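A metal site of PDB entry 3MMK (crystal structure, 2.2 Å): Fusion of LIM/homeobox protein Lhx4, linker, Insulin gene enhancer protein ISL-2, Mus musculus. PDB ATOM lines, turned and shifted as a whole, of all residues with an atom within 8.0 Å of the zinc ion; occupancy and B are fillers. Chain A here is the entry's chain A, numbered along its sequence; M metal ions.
The backbone NH of Glu 121 lies close to the side-chain sulfur of Cys 119, 3.8 Å away.
The side-chain sulfur (SG) of Cys 99 lies close to the backbone NH (N) of Arg 101 (3.4 Å).
N of Ile 98 lies close to SG of Cys 96, 3.4 Å away.
The backbone NH (N) of Cys 96 is in hydrogen-bond range of the backbone carbonyl oxygen (O) of Arg 101, 3.0 Å away.
Within 4 Å of the zinc ion: Cys 96, Cys 99, Cys 119 and Asp 122.
The nearest printed residue that does not touch the zinc ion is Ile 98 (4.6 Å).
The zinc ion is bound by OD2 of Asp 122 (2.2 Å), SG of Cys 119 (2.4 Å), SG of Cys 99 (2.4 Å) and SG of Cys 96 (2.4 Å).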
ATOM      1  N   ALA A  95      -4.731   7.809   2.273  1.00  0.00           N
ATOM      2  CA  ALA A  95      -3.807   8.938   2.383  1.00  0.00           C
ATOM      3  C   ALA A  95      -2.954   9.079   1.132  1.00  0.00           C
ATOM      4  O   ALA A  95      -2.683   8.105   0.440  1.00  0.00           O
ATOM      5  CB  ALA A  95      -2.917   8.754   3.607  1.00  0.00           C
ATOM      6  N   CYS A  96      -2.542  10.312   0.843  1.00  0.00           N
ATOM      7  CA  CYS A  96      -1.713  10.583  -0.331  1.00  0.00           C
ATOM      8  C   CYS A  96      -0.325   9.976  -0.161  1.00  0.00           C
ATOM      9  O   CYS A  96       0.330  10.166   0.866  1.00  0.00           O
ATOM     10  CB  CYS A  96      -1.612  12.086  -0.556  1.00  0.00           C
ATOM     11  SG  CYS A  96      -0.471  12.565  -1.865  1.00  0.00           S
ATOM     12  N   ILE A  97       0.131   9.251  -1.179  1.00  0.00           N
ATOM     13  CA  ILE A  97       1.425   8.569  -1.131  1.00  0.00           C
ATOM     14  C   ILE A  97       2.612   9.538  -1.179  1.00  0.00           C
ATOM     15  O   ILE A  97       3.716   9.179  -0.766  1.00  0.00           O
ATOM     16  CB  ILE A  97       1.582   7.556  -2.286  1.00  0.00           C
ATOM     17  CG1 ILE A  97       1.646   8.285  -3.630  1.00  0.00           C
ATOM     18  CG2 ILE A  97       0.450   6.553  -2.280  1.00  0.00           C
ATOM     19  CD1 ILE A  97       1.945   7.376  -4.805  1.00  0.00           C
ATOM     20  N   ILE A  98       2.386  10.734  -1.694  1.00  0.00           N
ATOM     21  CA  ILE A  98       3.447  11.733  -1.800  1.00  0.00           C
ATOM     22  C   ILE A  98       3.611  12.563  -0.534  1.00  0.00           C
ATOM     23  O   ILE A  98       4.718  12.652   0.002  1.00  0.00           O
ATOM     24  CB  ILE A  98       3.235  12.670  -3.005  1.00  0.00           C
ATOM     25  CG1 ILE A  98       3.548  11.947  -4.315  1.00  0.00           C
ATOM     26  CG2 ILE A  98       4.117  13.901  -2.875  1.00  0.00           C
ATOM     27  CD1 ILE A  98       3.384  12.828  -5.544  1.00  0.00           C
ATOM     28  N   CYS A  99       2.533  13.173  -0.064  1.00  0.00           N
ATOM     29  CA  CYS A  99       2.617  14.060   1.096  1.00  0.00           C
ATOM     30  C   CYS A  99       2.219  13.381   2.396  1.00  0.00           C
ATOM     31  O   CYS A  99       2.358  13.959   3.480  1.00  0.00           O
ATOM     32  CB  CYS A  99       1.763  15.316   0.882  1.00  0.00           C
ATOM     33  SG  CYS A  99      -0.020  15.014   0.952  1.00  0.00           S
ATOM     34  N   ASN A 100       1.711  12.157   2.293  1.00  0.00           N
ATOM     35  CA  ASN A 100       1.313  11.383   3.472  1.00  0.00           C
ATOM     36  C   ASN A 100       0.137  11.977   4.248  1.00  0.00           C
ATOM     37  O   ASN A 100      -0.192  11.504   5.335  1.00  0.00           O
ATOM     38  CB  ASN A 100       2.515  11.164   4.395  1.00  0.00           C
ATOM     39  CG  ASN A 100       3.636  10.400   3.725  1.00  0.00           C
ATOM     40  OD1 ASN A 100       3.446   9.281   3.273  1.00  0.00           O
ATOM     41  ND2 ASN A 100       4.818  11.017   3.676  1.00  0.00           N
ATOM     42  N   ARG A 101      -0.500  13.004   3.693  1.00  0.00           N
ATOM     43  CA  ARG A 101      -1.654  13.607   4.331  1.00  0.00           C
ATOM     44  C   ARG A 101      -2.907  12.742   4.156  1.00  0.00           C
ATOM     45  O   ARG A 101      -3.216  12.294   3.044  1.00  0.00           O
ATOM     46  CB  ARG A 101      -1.905  15.016   3.788  1.00  0.00           C
ATOM     47  CG  ARG A 101      -3.097  15.733   4.416  1.00  0.00           C
ATOM     48  N   GLN A 102      -3.638  12.507   5.242  1.00  0.00           N
ATOM     49  CA  GLN A 102      -4.875  11.754   5.184  1.00  0.00           C
ATOM     50  C   GLN A 102      -5.939  12.479   4.379  1.00  0.00           C
ATOM     51  O   GLN A 102      -6.154  13.676   4.558  1.00  0.00           O
ATOM     52  CB  GLN A 102      -5.411  11.450   6.578  1.00  0.00           C
ATOM     53  CG  GLN A 102      -4.906  10.152   7.170  1.00  0.00           C
ATOM     54  CD  GLN A 102      -5.300   9.984   8.630  1.00  0.00           C
ATOM     55  OE1 GLN A 102      -6.286   9.320   8.948  1.00  0.00           O
ATOM     56  NE2 GLN A 102      -4.536  10.607   9.524  1.00  0.00           N
ATOM     57  N   LEU A 103      -6.600  11.755   3.480  1.00  0.00           N
ATOM     58  CA  LEU A 103      -7.693  12.321   2.706  1.00  0.00           C
ATOM     59  C   LEU A 103      -8.967  12.348   3.543  1.00  0.00           C
ATOM     60  O   LEU A 103      -9.241  11.418   4.304  1.00  0.00           O
ATOM     61  CB  LEU A 103      -7.902  11.516   1.411  1.00  0.00           C
ATOM     62  CG  LEU A 103      -6.723  11.572   0.445  1.00  0.00           C
ATOM     63  CD1 LEU A 103      -6.863  10.547  -0.688  1.00  0.00           C
ATOM     64  CD2 LEU A 103      -6.576  12.977  -0.108  1.00  0.00           C
ATOM     65  N   GLU A 108     -10.303  16.151  -3.056  1.00  0.00           N
ATOM     66  CA  GLU A 108     -10.100  15.761  -4.444  1.00  0.00           C
ATOM     67  C   GLU A 108      -8.768  15.040  -4.566  1.00  0.00           C
ATOM     68  O   GLU A 108      -7.739  15.547  -4.135  1.00  0.00           O
ATOM     69  CB  GLU A 108     -10.138  16.994  -5.345  1.00  0.00           C
ATOM     70  CG  GLU A 108     -11.467  17.727  -5.294  1.00  0.00           C
ATOM     71  CD  GLU A 108     -11.381  19.131  -5.862  1.00  0.00           C
ATOM     72  OE1 GLU A 108     -10.277  19.709  -5.850  1.00  0.00           O
ATOM     73  OE2 GLU A 108     -12.423  19.650  -6.308  1.00  0.00           O
ATOM     74  N   LEU A 117      -2.960   6.192  -3.917  1.00  0.00           N
ATOM     75  CA  LEU A 117      -3.751   7.416  -3.831  1.00  0.00           C
ATOM     76  C   LEU A 117      -2.853   8.653  -3.851  1.00  0.00           C
ATOM     77  O   LEU A 117      -1.851   8.704  -3.157  1.00  0.00           O
ATOM     78  CB  LEU A 117      -4.586   7.420  -2.552  1.00  0.00           C
ATOM     79  CG  LEU A 117      -5.501   6.208  -2.338  1.00  0.00           C
ATOM     80  CD1 LEU A 117      -5.813   6.048  -0.868  1.00  0.00           C
ATOM     81  CD2 LEU A 117      -6.777   6.368  -3.149  1.00  0.00           C
ATOM     82  N   VAL A 118      -3.241   9.633  -4.660  1.00  0.00           N
ATOM     83  CA  VAL A 118      -2.495  10.890  -4.756  1.00  0.00           C
ATOM     84  C   VAL A 118      -3.430  12.083  -4.623  1.00  0.00           C
ATOM     85  O   VAL A 118      -4.378  12.212  -5.391  1.00  0.00           O
ATOM     86  CB  VAL A 118      -1.781  11.002  -6.104  1.00  0.00           C
ATOM     87  CG1 VAL A 118      -0.818  12.178  -6.083  1.00  0.00           C
ATOM     88  CG2 VAL A 118      -1.064   9.710  -6.441  1.00  0.00           C
ATOM     89  N   CYS A 119      -3.149  12.968  -3.665  1.00  0.00           N
ATOM     90  CA  CYS A 119      -3.964  14.173  -3.503  1.00  0.00           C
ATOM     91  C   CYS A 119      -3.911  14.982  -4.791  1.00  0.00           C
ATOM     92  O   CYS A 119      -2.959  14.860  -5.567  1.00  0.00           O
ATOM     93  CB  CYS A 119      -3.502  15.015  -2.300  1.00  0.00           C
ATOM     94  SG  CYS A 119      -2.095  16.118  -2.614  1.00  0.00           S
ATOM     95  N   LYS A 120      -4.928  15.797  -5.030  1.00  0.00           N
ATOM     96  CA  LYS A 120      -5.031  16.550  -6.277  1.00  0.00           C
ATOM     97  C   LYS A 120      -3.813  17.436  -6.531  1.00  0.00           C
ATOM     98  O   LYS A 120      -3.265  17.435  -7.640  1.00  0.00           O
ATOM     99  CB  LYS A 120      -6.299  17.401  -6.283  1.00  0.00           C
ATOM    100  CG  LYS A 120      -6.389  18.372  -7.456  1.00  0.00           C
ATOM    101  CD  LYS A 120      -7.665  19.188  -7.386  1.00  0.00           C
ATOM    102  CE  LYS A 120      -7.816  20.126  -8.576  1.00  0.00           C
ATOM    103  NZ  LYS A 120      -6.723  21.136  -8.611  1.00  0.00           N
ATOM    104  N   GLU A 121      -3.401  18.187  -5.513  1.00  0.00           N
ATOM    105  CA  GLU A 121      -2.286  19.120  -5.653  1.00  0.00           C
ATOM    106  C   GLU A 121      -0.986  18.431  -6.068  1.00  0.00           C
ATOM    107  O   GLU A 121      -0.322  18.853  -7.029  1.00  0.00           O
ATOM    108  CB  GLU A 121      -2.082  19.912  -4.360  1.00  0.00           C
ATOM    109  CG  GLU A 121      -0.805  20.732  -4.338  1.00  0.00           C
ATOM    110  CD  GLU A 121      -0.721  21.662  -3.154  1.00  0.00           C
ATOM    111  OE1 GLU A 121      -1.644  22.488  -2.979  1.00  0.00           O
ATOM    112  OE2 GLU A 121       0.259  21.566  -2.386  1.00  0.00           O
ATOM    113  N   ASP A 122      -0.608  17.374  -5.361  1.00  0.00           N
ATOM    114  CA  ASP A 122       0.620  16.648  -5.662  1.00  0.00           C
ATOM    115  C   ASP A 122       0.554  15.895  -6.991  1.00  0.00           C
ATOM    116  O   ASP A 122       1.557  15.791  -7.692  1.00  0.00           O
ATOM    117  CB  ASP A 122       0.964  15.673  -4.532  1.00  0.00           C
ATOM    118  CG  ASP A 122       1.478  16.385  -3.308  1.00  0.00           C
ATOM    119  OD1 ASP A 122       1.909  17.551  -3.454  1.00  0.00           O
ATOM    120  OD2 ASP A 122       1.442  15.795  -2.213  1.00  0.00           O
ATOM    121  N   TYR A 123      -0.614  15.381  -7.341  1.00  0.00           N
ATOM    122  CA  TYR A 123      -0.739  14.702  -8.627  1.00  0.00           C
ATOM    123  C   TYR A 123      -0.491  15.698  -9.749  1.00  0.00           C
ATOM    124  O   TYR A 123       0.315  15.460 -10.642  1.00  0.00           O
ATOM    125  CB  TYR A 123      -2.111  14.060  -8.779  1.00  0.00           C
ATOM    126  CG  TYR A 123      -2.276  13.325 -10.088  1.00  0.00           C
ATOM    127  CD1 TYR A 123      -1.959  11.972 -10.195  1.00  0.00           C
ATOM    128  CD2 TYR A 123      -2.747  13.977 -11.214  1.00  0.00           C
ATOM    129  CE1 TYR A 123      -2.112  11.305 -11.393  1.00  0.00           C
ATOM    130  CE2 TYR A 123      -2.898  13.311 -12.422  1.00  0.00           C
ATOM    131  CZ  TYR A 123      -2.582  11.969 -12.496  1.00  0.00           C
ATOM    132  OH  TYR A 123      -2.726  11.304 -13.692  1.00  0.00           O
HETATM  133 ZN    ZN M   1      -0.422  14.941  -1.427  1.00  0.00          ZN
